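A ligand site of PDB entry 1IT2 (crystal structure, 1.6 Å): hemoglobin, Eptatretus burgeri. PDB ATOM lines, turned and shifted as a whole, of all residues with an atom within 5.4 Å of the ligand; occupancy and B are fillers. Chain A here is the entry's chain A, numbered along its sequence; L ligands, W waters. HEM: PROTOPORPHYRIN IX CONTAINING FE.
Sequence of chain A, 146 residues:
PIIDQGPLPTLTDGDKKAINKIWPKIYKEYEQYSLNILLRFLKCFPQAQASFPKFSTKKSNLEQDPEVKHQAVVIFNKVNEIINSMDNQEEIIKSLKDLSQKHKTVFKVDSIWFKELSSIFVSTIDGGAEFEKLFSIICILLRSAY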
ATOM      1  N   PHE A  41      -4.501 -29.076  21.878  1.00  0.00           N
ATOM      2  CA  PHE A  41      -3.529 -30.098  22.264  1.00  0.00           C
ATOM      3  C   PHE A  41      -4.036 -30.882  23.479  1.00  0.00           C
ATOM      4  O   PHE A  41      -3.963 -32.105  23.498  1.00  0.00           O
ATOM      5  CB  PHE A  41      -2.178 -29.456  22.563  1.00  0.00           C
ATOM      6  CG  PHE A  41      -1.157 -30.402  23.152  1.00  0.00           C
ATOM      7  CD1 PHE A  41      -0.709 -31.502  22.426  1.00  0.00           C
ATOM      8  CD2 PHE A  41      -0.636 -30.177  24.432  1.00  0.00           C
ATOM      9  CE1 PHE A  41       0.252 -32.364  22.972  1.00  0.00           C
ATOM     10  CE2 PHE A  41       0.316 -31.036  24.977  1.00  0.00           C
ATOM     11  CZ  PHE A  41       0.754 -32.132  24.242  1.00  0.00           C
ATOM     12  N   ALA A  48      -1.755 -35.501  28.497  1.00  0.00           N
ATOM     13  CA  ALA A  48      -0.608 -34.589  28.506  1.00  0.00           C
ATOM     14  C   ALA A  48      -0.771 -33.493  29.556  1.00  0.00           C
ATOM     15  O   ALA A  48       0.194 -32.819  29.921  1.00  0.00           O
ATOM     16  CB  ALA A  48      -0.421 -33.967  27.116  1.00  0.00           C
ATOM     17  N   SER A  51       1.557 -33.056  32.525  1.00  0.00           N
ATOM     18  CA  SER A  51       2.872 -32.452  32.314  1.00  0.00           C
ATOM     19  C   SER A  51       2.945 -30.978  32.703  1.00  0.00           C
ATOM     20  O   SER A  51       4.013 -30.361  32.654  1.00  0.00           O
ATOM     21  CB  SER A  51       3.296 -32.605  30.853  1.00  0.00           C
ATOM     22  OG  SER A  51       3.431 -33.962  30.496  1.00  0.00           O
ATOM     23  N   PHE A  52       1.810 -30.403  33.104  1.00  0.00           N
ATOM     24  CA  PHE A  52       1.762 -28.990  33.491  1.00  0.00           C
ATOM     25  C   PHE A  52       1.225 -28.876  34.922  1.00  0.00           C
ATOM     26  O   PHE A  52       0.036 -28.627  35.140  1.00  0.00           O
ATOM     27  CB  PHE A  52       0.838 -28.201  32.555  1.00  0.00           C
ATOM     28  CG  PHE A  52       1.162 -28.337  31.092  1.00  0.00           C
ATOM     29  CD1 PHE A  52       0.523 -29.284  30.305  1.00  0.00           C
ATOM     30  CD2 PHE A  52       2.061 -27.455  30.481  1.00  0.00           C
ATOM     31  CE1 PHE A  52       0.757 -29.366  28.935  1.00  0.00           C
ATOM     32  CE2 PHE A  52       2.308 -27.529  29.102  1.00  0.00           C
ATOM     33  CZ  PHE A  52       1.658 -28.475  28.336  1.00  0.00           C
ATOM     34  N   PRO A  53       2.104 -29.066  35.927  1.00  0.00           N
ATOM     35  CA  PRO A  53       1.674 -28.977  37.329  1.00  0.00           C
ATOM     36  C   PRO A  53       0.890 -27.720  37.705  1.00  0.00           C
ATOM     37  O   PRO A  53       0.005 -27.771  38.556  1.00  0.00           O
ATOM     38  CB  PRO A  53       2.990 -29.090  38.121  1.00  0.00           C
ATOM     39  CG  PRO A  53       4.079 -28.866  37.128  1.00  0.00           C
ATOM     40  CD  PRO A  53       3.540 -29.354  35.816  1.00  0.00           C
ATOM     41  N   LYS A  54       1.191 -26.599  37.055  1.00  0.00           N
ATOM     42  CA  LYS A  54       0.503 -25.337  37.355  1.00  0.00           C
ATOM     43  C   LYS A  54      -0.997 -25.342  37.035  1.00  0.00           C
ATOM     44  O   LYS A  54      -1.716 -24.454  37.471  1.00  0.00           O
ATOM     45  CB  LYS A  54       1.221 -24.167  36.670  1.00  0.00           C
ATOM     46  CG  LYS A  54       2.636 -23.963  37.232  1.00  0.00           C
ATOM     47  CD  LYS A  54       3.284 -22.662  36.811  1.00  0.00           C
ATOM     48  CE  LYS A  54       4.588 -22.476  37.577  1.00  0.00           C
ATOM     49  NZ  LYS A  54       5.390 -21.333  37.084  1.00  0.00           N
ATOM     50  N   GLN A  71       0.777 -20.275  29.844  1.00  0.00           N
ATOM     51  CA  GLN A  71       1.578 -21.364  29.267  1.00  0.00           C
ATOM     52  C   GLN A  71       1.494 -21.288  27.740  1.00  0.00           C
ATOM     53  O   GLN A  71       2.505 -21.416  27.045  1.00  0.00           O
ATOM     54  CB  GLN A  71       1.061 -22.717  29.738  1.00  0.00           C
ATOM     55  CG  GLN A  71       1.847 -23.899  29.190  1.00  0.00           C
ATOM     56  CD  GLN A  71       3.288 -23.910  29.667  1.00  0.00           C
ATOM     57  OE1 GLN A  71       3.577 -24.283  30.805  1.00  0.00           O
ATOM     58  NE2 GLN A  71       4.208 -23.501  28.799  1.00  0.00           N
ATOM     59  N   VAL A  74       3.540 -18.314  26.260  1.00  0.00           N
ATOM     60  CA  VAL A  74       4.975 -18.474  26.447  1.00  0.00           C
ATOM     61  C   VAL A  74       5.527 -19.361  25.318  1.00  0.00           C
ATOM     62  O   VAL A  74       6.585 -19.078  24.734  1.00  0.00           O
ATOM     63  CB  VAL A  74       5.258 -19.086  27.839  1.00  0.00           C
ATOM     64  CG1 VAL A  74       6.643 -19.631  27.887  1.00  0.00           C
ATOM     65  CG2 VAL A  74       5.093 -18.035  28.914  1.00  0.00           C
ATOM     66  N   ILE A  75       4.801 -20.417  24.989  1.00  0.00           N
ATOM     67  CA  ILE A  75       5.189 -21.331  23.920  1.00  0.00           C
ATOM     68  C   ILE A  75       5.116 -20.593  22.573  1.00  0.00           C
ATOM     69  O   ILE A  75       6.041 -20.621  21.765  1.00  0.00           O
ATOM     70  CB  ILE A  75       4.245 -22.565  23.882  1.00  0.00           C
ATOM     71  CG1 ILE A  75       4.500 -23.443  25.120  1.00  0.00           C
ATOM     72  CG2 ILE A  75       4.435 -23.343  22.579  1.00  0.00           C
ATOM     73  CD1 ILE A  75       3.551 -24.606  25.272  1.00  0.00           C
ATOM     74  N   LYS A  78       7.923 -18.095  21.968  1.00  0.00           N
ATOM     75  CA  LYS A  78       9.204 -18.700  21.651  1.00  0.00           C
ATOM     76  C   LYS A  78       9.252 -18.975  20.149  1.00  0.00           C
ATOM     77  O   LYS A  78      10.253 -18.717  19.469  1.00  0.00           O
ATOM     78  CB  LYS A  78       9.399 -20.010  22.412  1.00  0.00           C
ATOM     79  CG  LYS A  78      10.800 -20.580  22.297  1.00  0.00           C
ATOM     80  CD  LYS A  78      11.677 -20.044  23.418  1.00  0.00           C
ATOM     81  CE  LYS A  78      12.556 -18.922  22.936  1.00  0.00           C
ATOM     82  NZ  LYS A  78      13.463 -19.413  21.870  1.00  0.00           N
ATOM     83  N   VAL A  79       8.159 -19.521  19.622  1.00  0.00           N
ATOM     84  CA  VAL A  79       8.080 -19.803  18.194  1.00  0.00           C
ATOM     85  C   VAL A  79       8.199 -18.483  17.428  1.00  0.00           C
ATOM     86  O   VAL A  79       8.885 -18.408  16.410  1.00  0.00           O
ATOM     87  CB  VAL A  79       6.737 -20.500  17.819  1.00  0.00           C
ATOM     88  CG1 VAL A  79       6.582 -20.573  16.301  1.00  0.00           C
ATOM     89  CG2 VAL A  79       6.691 -21.904  18.436  1.00  0.00           C
ATOM     90  N   LEU A  99      16.843 -24.399  26.320  1.00  0.00           N
ATOM     91  CA  LEU A  99      15.449 -24.634  26.672  1.00  0.00           C
ATOM     92  C   LEU A  99      15.188 -26.134  26.785  1.00  0.00           C
ATOM     93  O   LEU A  99      14.395 -26.573  27.624  1.00  0.00           O
ATOM     94  CB  LEU A  99      14.531 -24.018  25.605  1.00  0.00           C
ATOM     95  CG  LEU A  99      13.042 -23.920  25.913  1.00  0.00           C
ATOM     96  CD1 LEU A  99      12.816 -23.232  27.264  1.00  0.00           C
ATOM     97  CD2 LEU A  99      12.353 -23.150  24.793  1.00  0.00           C
ATOM     98  N   LYS A 102      16.215 -27.307  30.139  1.00  0.00           N
ATOM     99  CA  LYS A 102      15.278 -26.889  31.175  1.00  0.00           C
ATOM    100  C   LYS A 102      14.032 -27.782  31.224  1.00  0.00           C
ATOM    101  O   LYS A 102      13.568 -28.142  32.300  1.00  0.00           O
ATOM    102  CB  LYS A 102      14.869 -25.425  30.957  1.00  0.00           C
ATOM    103  CG  LYS A 102      15.119 -24.556  32.181  1.00  0.00           C
ATOM    104  CD  LYS A 102      14.304 -23.277  32.134  1.00  0.00           C
ATOM    105  CE  LYS A 102      13.976 -22.778  33.540  1.00  0.00           C
ATOM    106  NZ  LYS A 102      14.006 -21.283  33.618  1.00  0.00           N
ATOM    107  N   HIS A 103      13.503 -28.145  30.059  1.00  0.00           N
ATOM    108  CA  HIS A 103      12.318 -29.008  29.994  1.00  0.00           C
ATOM    109  C   HIS A 103      12.642 -30.388  30.550  1.00  0.00           C
ATOM    110  O   HIS A 103      11.796 -31.035  31.161  1.00  0.00           O
ATOM    111  CB  HIS A 103      11.823 -29.146  28.554  1.00  0.00           C
ATOM    112  CG  HIS A 103      11.018 -27.971  28.012  1.00  0.00           C
ATOM    113  ND1 HIS A 103      11.577 -26.724  27.701  1.00  0.00           N
ATOM    114  CD2 HIS A 103       9.627 -27.951  27.840  1.00  0.00           C
ATOM    115  CE1 HIS A 103      10.509 -25.975  27.359  1.00  0.00           C
ATOM    116  NE2 HIS A 103       9.407 -26.639  27.432  1.00  0.00           N
ATOM    117  N   PHE A 107      11.582 -28.767  34.213  1.00  0.00           N
ATOM    118  CA  PHE A 107      10.149 -28.981  34.002  1.00  0.00           C
ATOM    119  C   PHE A 107       9.782 -30.456  33.981  1.00  0.00           C
ATOM    120  O   PHE A 107       8.615 -30.818  34.118  1.00  0.00           O
ATOM    121  CB  PHE A 107       9.694 -28.313  32.700  1.00  0.00           C
ATOM    122  CG  PHE A 107      10.078 -26.858  32.597  1.00  0.00           C
ATOM    123  CD1 PHE A 107      10.354 -26.280  31.368  1.00  0.00           C
ATOM    124  CD2 PHE A 107      10.191 -26.078  33.743  1.00  0.00           C
ATOM    125  CE1 PHE A 107      10.738 -24.941  31.272  1.00  0.00           C
ATOM    126  CE2 PHE A 107      10.574 -24.741  33.667  1.00  0.00           C
ATOM    127  CZ  PHE A 107      10.847 -24.172  32.427  1.00  0.00           C
ATOM    128  N   VAL A 109       9.563 -32.684  31.600  1.00  0.00           N
ATOM    129  CA  VAL A 109       8.604 -32.989  30.553  1.00  0.00           C
ATOM    130  C   VAL A 109       9.131 -34.109  29.658  1.00  0.00           C
ATOM    131  O   VAL A 109      10.323 -34.160  29.353  1.00  0.00           O
ATOM    132  CB  VAL A 109       8.336 -31.719  29.694  1.00  0.00           C
ATOM    133  CG1 VAL A 109       7.604 -32.075  28.409  1.00  0.00           C
ATOM    134  CG2 VAL A 109       7.545 -30.696  30.515  1.00  0.00           C
ATOM    135  N   TRP A 113       6.228 -35.327  23.707  1.00  0.00           N
ATOM    136  CA  TRP A 113       5.125 -34.397  23.485  1.00  0.00           C
ATOM    137  C   TRP A 113       5.389 -33.236  22.526  1.00  0.00           C
ATOM    138  O   TRP A 113       4.460 -32.757  21.886  1.00  0.00           O
ATOM    139  CB  TRP A 113       4.637 -33.836  24.830  1.00  0.00           C
ATOM    140  CG  TRP A 113       3.905 -34.856  25.674  1.00  0.00           C
ATOM    141  CD1 TRP A 113       4.236 -35.257  26.942  1.00  0.00           C
ATOM    142  CD2 TRP A 113       2.742 -35.612  25.300  1.00  0.00           C
ATOM    143  NE1 TRP A 113       3.357 -36.226  27.372  1.00  0.00           N
ATOM    144  CE2 TRP A 113       2.426 -36.462  26.384  1.00  0.00           C
ATOM    145  CE3 TRP A 113       1.938 -35.653  24.150  1.00  0.00           C
ATOM    146  CZ2 TRP A 113       1.347 -37.349  26.361  1.00  0.00           C
ATOM    147  CZ3 TRP A 113       0.860 -36.540  24.127  1.00  0.00           C
ATOM    148  CH2 TRP A 113       0.580 -37.370  25.225  1.00  0.00           C
ATOM    149  N   PHE A 114       6.641 -32.785  22.414  1.00  0.00           N
ATOM    150  CA  PHE A 114       6.952 -31.638  21.546  1.00  0.00           C
ATOM    151  C   PHE A 114       6.369 -31.755  20.125  1.00  0.00           C
ATOM    152  O   PHE A 114       5.737 -30.822  19.633  1.00  0.00           O
ATOM    153  CB  PHE A 114       8.475 -31.450  21.446  1.00  0.00           C
ATOM    154  CG  PHE A 114       9.137 -31.163  22.760  1.00  0.00           C
ATOM    155  CD1 PHE A 114      10.278 -31.865  23.151  1.00  0.00           C
ATOM    156  CD2 PHE A 114       8.619 -30.198  23.627  1.00  0.00           C
ATOM    157  CE1 PHE A 114      10.892 -31.606  24.379  1.00  0.00           C
ATOM    158  CE2 PHE A 114       9.223 -29.937  24.865  1.00  0.00           C
ATOM    159  CZ  PHE A 114      10.363 -30.647  25.235  1.00  0.00           C
ATOM    160  N   LEU A 117       2.409 -31.460  20.092  1.00  0.00           N
ATOM    161  CA  LEU A 117       1.885 -30.095  20.231  1.00  0.00           C
ATOM    162  C   LEU A 117       2.170 -29.334  18.933  1.00  0.00           C
ATOM    163  O   LEU A 117       1.330 -28.595  18.438  1.00  0.00           O
ATOM    164  CB  LEU A 117       2.549 -29.385  21.413  1.00  0.00           C
ATOM    165  CG  LEU A 117       2.074 -27.946  21.684  1.00  0.00           C
ATOM    166  CD1 LEU A 117       2.182 -27.627  23.168  1.00  0.00           C
ATOM    167  CD2 LEU A 117       2.918 -26.972  20.880  1.00  0.00           C
ATOM    168  N   SER A 118       3.369 -29.523  18.390  1.00  0.00           N
ATOM    169  CA  SER A 118       3.773 -28.854  17.157  1.00  0.00           C
ATOM    170  C   SER A 118       2.853 -29.172  15.969  1.00  0.00           C
ATOM    171  O   SER A 118       2.574 -28.290  15.144  1.00  0.00           O
ATOM    172  CB  SER A 118       5.211 -29.225  16.805  1.00  0.00           C
ATOM    173  OG  SER A 118       6.110 -28.651  17.750  1.00  0.00           O
ATOM    174  N   PHE A 121      -0.109 -27.196  16.362  1.00  0.00           N
ATOM    175  CA  PHE A 121       0.253 -25.792  16.132  1.00  0.00           C
ATOM    176  C   PHE A 121       0.143 -25.544  14.624  1.00  0.00           C
ATOM    177  O   PHE A 121      -0.496 -24.594  14.174  1.00  0.00           O
ATOM    178  CB  PHE A 121       1.695 -25.531  16.601  1.00  0.00           C
ATOM    179  CG  PHE A 121       2.008 -24.088  16.897  1.00  0.00           C
ATOM    180  CD1 PHE A 121       1.874 -23.100  15.920  1.00  0.00           C
ATOM    181  CD2 PHE A 121       2.477 -23.711  18.162  1.00  0.00           C
ATOM    182  CE1 PHE A 121       2.211 -21.764  16.184  1.00  0.00           C
ATOM    183  CE2 PHE A 121       2.813 -22.377  18.437  1.00  0.00           C
ATOM    184  CZ  PHE A 121       2.686 -21.399  17.448  1.00  0.00           C
ATOM    185  N   PHE A 135       9.100 -26.391  12.448  1.00  0.00           N
ATOM    186  CA  PHE A 135       8.831 -27.097  13.693  1.00  0.00           C
ATOM    187  C   PHE A 135       9.681 -28.350  13.864  1.00  0.00           C
ATOM    188  O   PHE A 135       9.837 -28.831  14.984  1.00  0.00           O
ATOM    189  CB  PHE A 135       7.333 -27.419  13.798  1.00  0.00           C
ATOM    190  CG  PHE A 135       6.538 -26.306  14.419  1.00  0.00           C
ATOM    191  CD1 PHE A 135       5.895 -25.351  13.626  1.00  0.00           C
ATOM    192  CD2 PHE A 135       6.487 -26.160  15.805  1.00  0.00           C
ATOM    193  CE1 PHE A 135       5.227 -24.267  14.209  1.00  0.00           C
ATOM    194  CE2 PHE A 135       5.829 -25.080  16.397  1.00  0.00           C
ATOM    195  CZ  PHE A 135       5.193 -24.136  15.594  1.00  0.00           C
ATOM    196  N   ILE A 138      12.716 -26.935  15.409  1.00  0.00           N
ATOM    197  CA  ILE A 138      12.373 -26.640  16.810  1.00  0.00           C
ATOM    198  C   ILE A 138      12.291 -27.902  17.685  1.00  0.00           C
ATOM    199  O   ILE A 138      12.850 -27.924  18.786  1.00  0.00           O
ATOM    200  CB  ILE A 138      11.013 -25.881  16.909  1.00  0.00           C
ATOM    201  CG1 ILE A 138      11.142 -24.515  16.251  1.00  0.00           C
ATOM    202  CG2 ILE A 138      10.599 -25.733  18.380  1.00  0.00           C
ATOM    203  CD1 ILE A 138       9.827 -23.752  16.151  1.00  0.00           C
ATOM    204  N   LEU A 142      14.589 -29.099  20.761  1.00  0.00           N
ATOM    205  CA  LEU A 142      13.985 -29.203  22.082  1.00  0.00           C
ATOM    206  C   LEU A 142      14.197 -30.610  22.671  1.00  0.00           C
ATOM    207  O   LEU A 142      14.149 -30.808  23.885  1.00  0.00           O
ATOM    208  CB  LEU A 142      12.479 -28.913  21.998  1.00  0.00           C
ATOM    209  CG  LEU A 142      12.068 -27.440  22.034  1.00  0.00           C
ATOM    210  CD1 LEU A 142      10.561 -27.315  21.859  1.00  0.00           C
ATOM    211  CD2 LEU A 142      12.533 -26.808  23.349  1.00  0.00           C
HETATM  212  CHA HEM L   1       7.834 -23.679  29.819  1.00  0.00           C
HETATM  213  CHB HEM L   1       8.457 -23.256  24.988  1.00  0.00           C
HETATM  214  CHC HEM L   1       6.327 -27.567  24.340  1.00  0.00           C
HETATM  215  CHD HEM L   1       5.685 -27.949  29.134  1.00  0.00           C
HETATM  216  C1A HEM L   1       8.223 -23.221  28.550  1.00  0.00           C
HETATM  217  C2A HEM L   1       8.869 -21.917  28.341  1.00  0.00           C
HETATM  218  C3A HEM L   1       9.045 -21.788  26.993  1.00  0.00           C
HETATM  219  C4A HEM L   1       8.476 -23.005  26.380  1.00  0.00           C
HETATM  220  CMA HEM L   1       9.733 -20.617  26.286  1.00  0.00           C
HETATM  221  CAA HEM L   1       9.282 -20.908  29.437  1.00  0.00           C
HETATM  222  CBA HEM L   1      10.745 -21.071  29.836  1.00  0.00           C
HETATM  223  CGA HEM L   1      11.109 -20.392  31.153  1.00  0.00           C
HETATM  224  O1A HEM L   1      12.307 -20.351  31.494  1.00  0.00           O
HETATM  225  O2A HEM L   1      10.195 -19.904  31.855  1.00  0.00           O
HETATM  226  C1B HEM L   1       8.001 -24.435  24.404  1.00  0.00           C
HETATM  227  C2B HEM L   1       7.940 -24.656  22.944  1.00  0.00           C
HETATM  228  C3B HEM L   1       7.307 -25.858  22.742  1.00  0.00           C
HETATM  229  C4B HEM L   1       7.012 -26.384  24.098  1.00  0.00           C
HETATM  230  CMB HEM L   1       8.538 -23.719  21.893  1.00  0.00           C
HETATM  231  CAB HEM L   1       7.010 -26.517  21.532  1.00  0.00           C
HETATM  232  CBB HEM L   1       6.777 -25.944  20.259  1.00  0.00           C
HETATM  233  C1C HEM L   1       6.000 -28.064  25.617  1.00  0.00           C
HETATM  234  C2C HEM L   1       5.208 -29.258  25.833  1.00  0.00           C
HETATM  235  C3C HEM L   1       5.014 -29.374  27.201  1.00  0.00           C
HETATM  236  C4C HEM L   1       5.698 -28.234  27.771  1.00  0.00           C
HETATM  237  CMC HEM L   1       4.750 -30.237  24.768  1.00  0.00           C
HETATM  238  CAC HEM L   1       4.323 -30.361  27.950  1.00  0.00           C
HETATM  239  CBC HEM L   1       3.727 -31.553  27.510  1.00  0.00           C
HETATM  240  C1D HEM L   1       6.210 -26.821  29.725  1.00  0.00           C
HETATM  241  C2D HEM L   1       6.165 -26.571  31.174  1.00  0.00           C
HETATM  242  C3D HEM L   1       6.774 -25.381  31.363  1.00  0.00           C
HETATM  243  C4D HEM L   1       7.183 -24.891  30.049  1.00  0.00           C
HETATM  244  CMD HEM L   1       5.605 -27.519  32.236  1.00  0.00           C
HETATM  245  CAD HEM L   1       7.018 -24.682  32.697  1.00  0.00           C
HETATM  246  CBD HEM L   1       5.963 -23.629  32.956  1.00  0.00           C
HETATM  247  CGD HEM L   1       6.190 -22.879  34.255  1.00  0.00           C
HETATM  248  O1D HEM L   1       6.551 -23.525  35.263  1.00  0.00           O
HETATM  249  O2D HEM L   1       5.994 -21.649  34.271  1.00  0.00           O
HETATM  250  NA  HEM L   1       8.032 -23.911  27.351  1.00  0.00           N
HETATM  251  NB  HEM L   1       7.464 -25.508  25.089  1.00  0.00           N
HETATM  252  NC  HEM L   1       6.333 -27.424  26.817  1.00  0.00           N
HETATM  253  ND  HEM L   1       6.864 -25.812  29.048  1.00  0.00           N
HETATM  254 FE   HEM L   1       7.379 -25.766  27.081  1.00  0.00          FE
HETATM  255  O   HOH W   1       5.589 -25.867  35.909  1.00  0.00           O
HETATM  256  O   HOH W   2      14.083 -20.090  29.368  1.00  0.00           O
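O1A of the ligand is in salt-bridge range of NZ of Lys 102. O2D of the ligand lies within salt-bridge range of NZ of Lys 54 (2.9 Å). An iron atom (FE) of the ligand is bound by a ring nitrogen (NE2) of His 103 (2.2 Å).
The backbone carbonyl oxygen of Leu 99 is in hydrogen-bond range of a ring nitrogen (ND1) of His 103. The backbone NH (N) of Phe 107 is in hydrogen-bond range of the backbone carbonyl oxygen (O) of Lys 102. O of Phe 114 sits at hydrogen-bond distance from OG of Ser 118, at 2.9 Å. O of His 103 lies within hydrogen-bond range of N of Val 109 (2.8 Å). The backbone carbonyl oxygen (O) of Ala 48 lies close to the side-chain hydroxyl (OG) of Ser 51 (3.5 Å).
Merely in contact with the ligand: Val 74 (3.2 Å), Gln 71 (3.3 Å), Ser 51 (3.3 Å), Phe 52 (3.3 Å), Phe 107 (3.5 Å), Lys 78 (3.5 Å), Phe 114 (3.6 Å), Val 109 (3.6 Å), Trp 113 (3.6 Å), Ile 75 (3.6 Å), Leu 142 (3.7 Å), Ser 118 (3.8 Å), Leu 99 (3.9 Å) and Leu 117 (3.996 Å). Hydrophobic or aromatic side chains that line the ligand: Phe 52, Val 74, Ile 75, Leu 99, His 103, Phe 107, Val 109, Trp 113, Phe 114, Leu 117 and Leu 142.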
